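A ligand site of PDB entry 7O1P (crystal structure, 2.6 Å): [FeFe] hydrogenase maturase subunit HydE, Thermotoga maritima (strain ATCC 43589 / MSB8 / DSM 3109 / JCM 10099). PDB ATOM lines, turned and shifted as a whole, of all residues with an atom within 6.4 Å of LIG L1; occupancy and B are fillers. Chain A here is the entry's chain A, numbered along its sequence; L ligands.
Lys 64 touches LIG L1.
Tyr 68 touches LIG L1 (CE1 to S2, 3.7 Å).
Leu 71 touches LIG L1.
Arg 72 touches LIG L1 (CA to S4, 3.9 Å).
Gly 108 touches LIG L1.
CG of Glu 109 touches S1 of LIG L1, 3.9 Å away.
Hydrophobic or aromatic side chains that line LIG L1: Tyr 68 and Leu 71.
Of the 21 residues printed, 9 come within 4 Å of LIG L1.
N of Lys 64 sits close to SG of Cys 62 (3.4 Å).
The guanidinium group (NE) of Arg 171 lies within hydrogen-bond range of the side-chain hydroxyl (OH) of Tyr 68, at 3.0 Å.
The side-chain sulfur (SG) of Cys 66 lies close to the guanidinium group (NE) of Arg 171.
The guanidinium group of Arg 72 is in hydrogen-bond range of the backbone carbonyl oxygen of Cys 66 (2.7 Å).
The side-chain sulfur (SG) of Cys 69 sits close to the backbone NH (N) of Leu 71 (3.3 Å).
The guanidinium group (NH2) of Arg 72 is in hydrogen-bond range of the backbone carbonyl oxygen (O) of Asn 65 (3.1 Å).
The backbone carbonyl oxygen of Lys 64 is in hydrogen-bond range of the backbone NH of Arg 73, at 2.8 Å.
The side-chain sulfur (SG) of Cys 66 sits close to the side-chain hydroxyl (OH) of Tyr 68.
The side-chain sulfur (SG) of Cys 69 binds an iron atom (FE1) of LIG L1 (2.3 Å).
FE2 of LIG L1 is bound by SG of Cys 62 (2.3 Å).
The backbone carbonyl oxygen (O) of Tyr 68 lies within hydrogen-bond range of a nitrogen (N4) of LG2 L2, 3.2 Å away.
A nitrogen (N1) of LG2 L2 sits close to the backbone carbonyl oxygen (O) of Ser 107 (3.3 Å).
The guanidinium group of Arg 179 lies within salt-bridge range of an oxygen (O2) of LG2 L2.
SG of Cys 66 binds FE3 of LIG L1, at 2.3 Å.
The backbone NH of Cys 66 sits close to a sulfur (S4) of LIG L1 (3.7 Å).
The side-chain carboxylate (OE1) of Glu 160 is in hydrogen-bond range of an oxygen (O5) of LG2 L2 (2.7 Å).
A nitrogen (N1) of LG2 L2 binds an iron atom (FE4) of LIG L1 (2.2 Å).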
ATOM      1  N   CYS A  62      -8.284 -14.439 -11.628  1.00  0.00           N
ATOM      2  CA  CYS A  62      -9.504 -13.706 -11.357  1.00  0.00           C
ATOM      3  C   CYS A  62      -9.758 -13.590  -9.857  1.00  0.00           C
ATOM      4  O   CYS A  62      -9.439 -14.497  -9.085  1.00  0.00           O
ATOM      5  CB  CYS A  62     -10.719 -14.344 -12.027  1.00  0.00           C
ATOM      6  SG  CYS A  62     -12.183 -13.292 -11.956  1.00  0.00           S
ATOM      7  N   ARG A  63     -10.348 -12.463  -9.474  1.00  0.00           N
ATOM      8  CA  ARG A  63     -10.674 -12.203  -8.071  1.00  0.00           C
ATOM      9  C   ARG A  63     -12.078 -12.664  -7.698  1.00  0.00           C
ATOM     10  O   ARG A  63     -12.361 -12.811  -6.507  1.00  0.00           O
ATOM     11  CB  ARG A  63     -10.545 -10.711  -7.775  1.00  0.00           C
ATOM     12  CG  ARG A  63     -11.589  -9.852  -8.467  1.00  0.00           C
ATOM     13  CD  ARG A  63     -11.330  -8.362  -8.247  1.00  0.00           C
ATOM     14  NE  ARG A  63     -12.332  -7.537  -8.921  1.00  0.00           N
ATOM     15  CZ  ARG A  63     -12.399  -6.211  -8.827  1.00  0.00           C
ATOM     16  NH1 ARG A  63     -11.526  -5.554  -8.079  1.00  0.00           N
ATOM     17  NH2 ARG A  63     -13.343  -5.550  -9.482  1.00  0.00           N
ATOM     18  N   LYS A  64     -12.948 -12.899  -8.684  1.00  0.00           N
ATOM     19  CA  LYS A  64     -14.316 -13.280  -8.403  1.00  0.00           C
ATOM     20  C   LYS A  64     -14.445 -14.804  -8.306  1.00  0.00           C
ATOM     21  O   LYS A  64     -13.480 -15.556  -8.445  1.00  0.00           O
ATOM     22  CB  LYS A  64     -15.250 -12.704  -9.466  1.00  0.00           C
ATOM     23  CG  LYS A  64     -15.620 -11.251  -9.202  1.00  0.00           C
ATOM     24  CD  LYS A  64     -16.550 -10.709 -10.276  1.00  0.00           C
ATOM     25  CE  LYS A  64     -17.187  -9.406  -9.834  1.00  0.00           C
ATOM     26  NZ  LYS A  64     -16.163  -8.376  -9.509  1.00  0.00           N
ATOM     27  N   ASN A  65     -15.669 -15.267  -8.051  1.00  0.00           N
ATOM     28  CA  ASN A  65     -15.939 -16.660  -7.736  1.00  0.00           C
ATOM     29  C   ASN A  65     -17.198 -17.138  -8.444  1.00  0.00           C
ATOM     30  O   ASN A  65     -18.004 -17.870  -7.867  1.00  0.00           O
ATOM     31  CB  ASN A  65     -16.069 -16.865  -6.234  1.00  0.00           C
ATOM     32  CG  ASN A  65     -15.693 -18.255  -5.791  1.00  0.00           C
ATOM     33  OD1 ASN A  65     -14.923 -18.956  -6.450  1.00  0.00           O
ATOM     34  ND2 ASN A  65     -16.220 -18.680  -4.636  1.00  0.00           N
ATOM     35  N   CYS A  66     -17.387 -16.717  -9.698  1.00  0.00           N
ATOM     36  CA  CYS A  66     -18.570 -17.104 -10.478  1.00  0.00           C
ATOM     37  C   CYS A  66     -18.711 -18.624 -10.498  1.00  0.00           C
ATOM     38  O   CYS A  66     -17.733 -19.342 -10.710  1.00  0.00           O
ATOM     39  CB  CYS A  66     -18.448 -16.554 -11.900  1.00  0.00           C
ATOM     40  SG  CYS A  66     -18.404 -14.750 -12.028  1.00  0.00           S
ATOM     41  N   LEU A  67     -19.931 -19.099 -10.248  1.00  0.00           N
ATOM     42  CA  LEU A  67     -20.164 -20.532 -10.082  1.00  0.00           C
ATOM     43  C   LEU A  67     -19.963 -21.299 -11.378  1.00  0.00           C
ATOM     44  O   LEU A  67     -19.588 -22.476 -11.343  1.00  0.00           O
ATOM     45  CB  LEU A  67     -21.577 -20.778  -9.543  1.00  0.00           C
ATOM     46  CG  LEU A  67     -21.776 -20.691  -8.030  1.00  0.00           C
ATOM     47  CD1 LEU A  67     -21.855 -19.243  -7.561  1.00  0.00           C
ATOM     48  CD2 LEU A  67     -23.020 -21.460  -7.598  1.00  0.00           C
ATOM     49  N   TYR A  68     -20.229 -20.669 -12.519  1.00  0.00           N
ATOM     50  CA  TYR A  68     -20.098 -21.357 -13.808  1.00  0.00           C
ATOM     51  C   TYR A  68     -18.668 -21.356 -14.335  1.00  0.00           C
ATOM     52  O   TYR A  68     -18.316 -22.265 -15.096  1.00  0.00           O
ATOM     53  CB  TYR A  68     -21.016 -20.701 -14.844  1.00  0.00           C
ATOM     54  CG  TYR A  68     -20.927 -19.175 -14.857  1.00  0.00           C
ATOM     55  CD1 TYR A  68     -19.943 -18.530 -15.598  1.00  0.00           C
ATOM     56  CD2 TYR A  68     -21.820 -18.408 -14.118  1.00  0.00           C
ATOM     57  CE1 TYR A  68     -19.856 -17.148 -15.607  1.00  0.00           C
ATOM     58  CE2 TYR A  68     -21.746 -17.032 -14.123  1.00  0.00           C
ATOM     59  CZ  TYR A  68     -20.758 -16.400 -14.870  1.00  0.00           C
ATOM     60  OH  TYR A  68     -20.688 -15.032 -14.875  1.00  0.00           O
ATOM     61  N   CYS A  69     -17.849 -20.384 -13.955  1.00  0.00           N
ATOM     62  CA  CYS A  69     -16.590 -20.129 -14.629  1.00  0.00           C
ATOM     63  C   CYS A  69     -15.446 -20.931 -14.007  1.00  0.00           C
ATOM     64  O   CYS A  69     -15.319 -21.017 -12.787  1.00  0.00           O
ATOM     65  CB  CYS A  69     -16.239 -18.638 -14.581  1.00  0.00           C
ATOM     66  SG  CYS A  69     -14.756 -18.228 -15.492  1.00  0.00           S
ATOM     67  N   GLY A  70     -14.602 -21.496 -14.870  1.00  0.00           N
ATOM     68  CA  GLY A  70     -13.445 -22.235 -14.413  1.00  0.00           C
ATOM     69  C   GLY A  70     -12.336 -21.368 -13.835  1.00  0.00           C
ATOM     70  O   GLY A  70     -11.456 -21.888 -13.147  1.00  0.00           O
ATOM     71  N   LEU A  71     -12.353 -20.059 -14.113  1.00  0.00           N
ATOM     72  CA  LEU A  71     -11.372 -19.139 -13.546  1.00  0.00           C
ATOM     73  C   LEU A  71     -11.767 -18.617 -12.174  1.00  0.00           C
ATOM     74  O   LEU A  71     -11.057 -17.761 -11.627  1.00  0.00           O
ATOM     75  CB  LEU A  71     -11.133 -17.959 -14.490  1.00  0.00           C
ATOM     76  CG  LEU A  71     -10.720 -18.214 -15.938  1.00  0.00           C
ATOM     77  CD1 LEU A  71     -10.206 -16.928 -16.572  1.00  0.00           C
ATOM     78  CD2 LEU A  71      -9.674 -19.314 -16.019  1.00  0.00           C
ATOM     79  N   ARG A  72     -12.887 -19.078 -11.615  1.00  0.00           N
ATOM     80  CA  ARG A  72     -13.309 -18.640 -10.290  1.00  0.00           C
ATOM     81  C   ARG A  72     -12.177 -18.851  -9.281  1.00  0.00           C
ATOM     82  O   ARG A  72     -11.411 -19.809  -9.387  1.00  0.00           O
ATOM     83  CB  ARG A  72     -14.565 -19.403  -9.863  1.00  0.00           C
ATOM     84  CG  ARG A  72     -14.370 -20.910  -9.770  1.00  0.00           C
ATOM     85  CD  ARG A  72     -15.686 -21.661  -9.806  1.00  0.00           C
ATOM     86  NE  ARG A  72     -16.671 -21.087  -8.894  1.00  0.00           N
ATOM     87  CZ  ARG A  72     -16.761 -21.406  -7.608  1.00  0.00           C
ATOM     88  NH1 ARG A  72     -15.932 -22.300  -7.085  1.00  0.00           N
ATOM     89  NH2 ARG A  72     -17.687 -20.836  -6.856  1.00  0.00           N
ATOM     90  N   ARG A  73     -12.095 -17.941  -8.307  1.00  0.00           N
ATOM     91  CA  ARG A  73     -10.923 -17.904  -7.433  1.00  0.00           C
ATOM     92  C   ARG A  73     -10.773 -19.170  -6.582  1.00  0.00           C
ATOM     93  O   ARG A  73      -9.687 -19.410  -6.043  1.00  0.00           O
ATOM     94  CB  ARG A  73     -10.976 -16.686  -6.516  1.00  0.00           C
ATOM     95  CG  ARG A  73     -12.048 -16.743  -5.436  1.00  0.00           C
ATOM     96  CD  ARG A  73     -11.924 -15.561  -4.478  1.00  0.00           C
ATOM     97  NE  ARG A  73     -13.002 -15.540  -3.497  1.00  0.00           N
ATOM     98  CZ  ARG A  73     -14.089 -14.786  -3.609  1.00  0.00           C
ATOM     99  NH1 ARG A  73     -14.260 -13.997  -4.665  1.00  0.00           N
ATOM    100  NH2 ARG A  73     -15.028 -14.820  -2.666  1.00  0.00           N
ATOM    101  N   SER A 107      -9.435 -10.976 -19.887  1.00  0.00           N
ATOM    102  CA  SER A 107      -8.825 -11.719 -18.784  1.00  0.00           C
ATOM    103  C   SER A 107      -9.862 -11.874 -17.691  1.00  0.00           C
ATOM    104  O   SER A 107     -10.933 -11.257 -17.726  1.00  0.00           O
ATOM    105  CB  SER A 107      -7.582 -10.995 -18.246  1.00  0.00           C
ATOM    106  OG  SER A 107      -7.935  -9.743 -17.688  1.00  0.00           O
ATOM    107  N   GLY A 108      -9.538 -12.710 -16.722  1.00  0.00           N
ATOM    108  CA  GLY A 108     -10.219 -12.631 -15.439  1.00  0.00           C
ATOM    109  C   GLY A 108      -9.931 -11.306 -14.775  1.00  0.00           C
ATOM    110  O   GLY A 108      -9.063 -10.539 -15.199  1.00  0.00           O
ATOM    111  N   GLU A 109     -10.676 -11.020 -13.719  1.00  0.00           N
ATOM    112  CA  GLU A 109     -10.479  -9.765 -13.005  1.00  0.00           C
ATOM    113  C   GLU A 109      -9.177  -9.819 -12.222  1.00  0.00           C
ATOM    114  O   GLU A 109      -9.148 -10.253 -11.073  1.00  0.00           O
ATOM    115  CB  GLU A 109     -11.664  -9.471 -12.092  1.00  0.00           C
ATOM    116  CG  GLU A 109     -13.001  -9.415 -12.827  1.00  0.00           C
ATOM    117  CD  GLU A 109     -14.061  -8.643 -12.085  1.00  0.00           C
ATOM    118  OE1 GLU A 109     -13.876  -8.364 -10.885  1.00  0.00           O
ATOM    119  OE2 GLU A 109     -15.085  -8.292 -12.717  1.00  0.00           O
ATOM    120  N   GLY A 137     -14.088  -7.250 -17.138  1.00  0.00           N
ATOM    121  CA  GLY A 137     -15.004  -7.354 -16.023  1.00  0.00           C
ATOM    122  C   GLY A 137     -15.387  -6.011 -15.439  1.00  0.00           C
ATOM    123  O   GLY A 137     -15.308  -4.965 -16.110  1.00  0.00           O
ATOM    124  N   GLU A 160     -24.827 -11.723 -18.778  1.00  0.00           N
ATOM    125  CA  GLU A 160     -24.862 -13.094 -18.250  1.00  0.00           C
ATOM    126  C   GLU A 160     -26.283 -13.611 -18.043  1.00  0.00           C
ATOM    127  O   GLU A 160     -26.618 -14.706 -18.510  1.00  0.00           O
ATOM    128  CB  GLU A 160     -24.063 -13.175 -16.946  1.00  0.00           C
ATOM    129  CG  GLU A 160     -22.678 -12.497 -16.970  1.00  0.00           C
ATOM    130  CD  GLU A 160     -21.643 -13.201 -17.839  1.00  0.00           C
ATOM    131  OE1 GLU A 160     -22.022 -14.040 -18.695  1.00  0.00           O
ATOM    132  OE2 GLU A 160     -20.435 -12.923 -17.671  1.00  0.00           O
ATOM    133  N   ARG A 171     -23.382 -15.351  -9.490  1.00  0.00           N
ATOM    134  CA  ARG A 171     -22.232 -14.470  -9.327  1.00  0.00           C
ATOM    135  C   ARG A 171     -22.334 -13.873  -7.930  1.00  0.00           C
ATOM    136  O   ARG A 171     -22.945 -12.822  -7.727  1.00  0.00           O
ATOM    137  CB  ARG A 171     -22.214 -13.402 -10.425  1.00  0.00           C
ATOM    138  CG  ARG A 171     -22.553 -13.972 -11.802  1.00  0.00           C
ATOM    139  CD  ARG A 171     -22.340 -12.966 -12.919  1.00  0.00           C
ATOM    140  NE  ARG A 171     -20.941 -12.600 -13.061  1.00  0.00           N
ATOM    141  CZ  ARG A 171     -20.487 -11.354 -12.978  1.00  0.00           C
ATOM    142  NH1 ARG A 171     -21.334 -10.354 -12.761  1.00  0.00           N
ATOM    143  NH2 ARG A 171     -19.196 -11.104 -13.109  1.00  0.00           N
ATOM    144  N   ARG A 179     -23.803  -4.992 -12.522  1.00  0.00           N
ATOM    145  CA  ARG A 179     -23.484  -5.317 -13.907  1.00  0.00           C
ATOM    146  C   ARG A 179     -24.184  -4.372 -14.871  1.00  0.00           C
ATOM    147  O   ARG A 179     -23.574  -3.880 -15.838  1.00  0.00           O
ATOM    148  CB  ARG A 179     -23.865  -6.761 -14.209  1.00  0.00           C
ATOM    149  CG  ARG A 179     -23.208  -7.358 -15.441  1.00  0.00           C
ATOM    150  CD  ARG A 179     -21.788  -7.813 -15.144  1.00  0.00           C
ATOM    151  NE  ARG A 179     -21.221  -8.636 -16.214  1.00  0.00           N
ATOM    152  CZ  ARG A 179     -19.983  -9.121 -16.209  1.00  0.00           C
ATOM    153  NH1 ARG A 179     -19.179  -8.856 -15.187  1.00  0.00           N
ATOM    154  NH2 ARG A 179     -19.550  -9.849 -17.219  1.00  0.00           N
ATOM    155  N   TYR A 302      -6.500 -21.050 -20.066  1.00  0.00           N
ATOM    156  CA  TYR A 302      -7.597 -20.084 -19.968  1.00  0.00           C
ATOM    157  C   TYR A 302      -8.908 -20.837 -20.151  1.00  0.00           C
ATOM    158  O   TYR A 302      -9.507 -20.852 -21.230  1.00  0.00           O
ATOM    159  CB  TYR A 302      -7.416 -18.979 -20.999  1.00  0.00           C
ATOM    160  CG  TYR A 302      -8.319 -17.783 -20.780  1.00  0.00           C
ATOM    161  CD1 TYR A 302      -7.926 -16.736 -19.959  1.00  0.00           C
ATOM    162  CD2 TYR A 302      -9.548 -17.700 -21.407  1.00  0.00           C
ATOM    163  CE1 TYR A 302      -8.752 -15.644 -19.758  1.00  0.00           C
ATOM    164  CE2 TYR A 302     -10.377 -16.606 -21.214  1.00  0.00           C
ATOM    165  CZ  TYR A 302      -9.969 -15.578 -20.393  1.00  0.00           C
ATOM    166  OH  TYR A 302     -10.786 -14.490 -20.196  1.00  0.00           O
ATOM    167  N   LEU A 304     -12.396 -20.794 -19.098  1.00  0.00           N
ATOM    168  CA  LEU A 304     -13.746 -20.457 -18.663  1.00  0.00           C
ATOM    169  C   LEU A 304     -14.612 -21.707 -18.646  1.00  0.00           C
ATOM    170  O   LEU A 304     -15.330 -21.976 -17.682  1.00  0.00           O
ATOM    171  CB  LEU A 304     -14.348 -19.396 -19.589  1.00  0.00           C
ATOM    172  CG  LEU A 304     -13.480 -18.187 -19.933  1.00  0.00           C
ATOM    173  CD1 LEU A 304     -14.099 -17.414 -21.079  1.00  0.00           C
ATOM    174  CD2 LEU A 304     -13.276 -17.291 -18.720  1.00  0.00           C
HETATM  175 FE1  LIG L   1     -14.953 -16.092 -14.779  1.00  0.00          FE
HETATM  176 FE2  LIG L   1     -13.869 -14.172 -13.230  1.00  0.00          FE
HETATM  177 FE3  LIG L   1     -16.539 -14.431 -13.334  1.00  0.00          FE
HETATM  178 FE4  LIG L   1     -15.131 -13.433 -15.498  1.00  0.00          FE
HETATM  179  S1  LIG L   1     -15.375 -12.448 -13.442  1.00  0.00           S
HETATM  180  S2  LIG L   1     -16.822 -14.993 -15.546  1.00  0.00           S
HETATM  181  S3  LIG L   1     -13.221 -14.700 -15.377  1.00  0.00           S
HETATM  182  S4  LIG L   1     -15.065 -15.990 -12.481  1.00  0.00           S
HETATM  183  N1  LG2 L   2     -13.850 -11.835 -16.267  1.00  0.00           N
HETATM  184  C1  LG2 L   2     -14.488 -11.038 -17.310  1.00  0.00           C
HETATM  185  C2  LG2 L   2     -14.053 -11.500 -18.703  1.00  0.00           C
HETATM  186  C3  LG2 L   2     -13.959 -13.005 -18.959  1.00  0.00           C
HETATM  187  S1  LG2 L   2     -15.465 -13.949 -18.638  1.00  0.00           S
HETATM  188  C4  LG2 L   2     -16.004 -11.097 -17.189  1.00  0.00           C
HETATM  189  O1  LG2 L   2     -16.546 -11.878 -16.398  1.00  0.00           O
HETATM  190  O2  LG2 L   2     -16.719 -10.379 -17.899  1.00  0.00           O
HETATM  191  C5  LG2 L   2     -15.863 -13.975 -20.404  1.00  0.00           C
HETATM  192  C6  LG2 L   2     -17.186 -14.655 -20.718  1.00  0.00           C
HETATM  193  O3  LG2 L   2     -17.072 -16.065 -20.766  1.00  0.00           O
HETATM  194  C7  LG2 L   2     -18.263 -14.370 -19.685  1.00  0.00           C
HETATM  195  O4  LG2 L   2     -19.000 -13.232 -20.042  1.00  0.00           O
HETATM  196  C8  LG2 L   2     -19.126 -15.606 -19.720  1.00  0.00           C
HETATM  197  O5  LG2 L   2     -20.350 -15.344 -20.375  1.00  0.00           O
HETATM  198  C9  LG2 L   2     -18.352 -16.621 -20.538  1.00  0.00           C
HETATM  199  N2  LG2 L   2     -18.293 -17.889 -19.785  1.00  0.00           N
HETATM  200  C10 LG2 L   2     -17.671 -18.075 -18.584  1.00  0.00           C
HETATM  201  N3  LG2 L   2     -17.848 -19.362 -18.209  1.00  0.00           N
HETATM  202  C11 LG2 L   2     -18.582 -19.994 -19.152  1.00  0.00           C
HETATM  203  C12 LG2 L   2     -19.049 -21.299 -19.257  1.00  0.00           C
HETATM  204  N4  LG2 L   2     -18.785 -22.193 -18.302  1.00  0.00           N
HETATM  205  N5  LG2 L   2     -19.794 -21.666 -20.354  1.00  0.00           N
HETATM  206  C13 LG2 L   2     -20.077 -20.748 -21.339  1.00  0.00           C
HETATM  207  N6  LG2 L   2     -19.606 -19.446 -21.226  1.00  0.00           N
HETATM  208  C14 LG2 L   2     -18.872 -19.071 -20.155  1.00  0.00           C
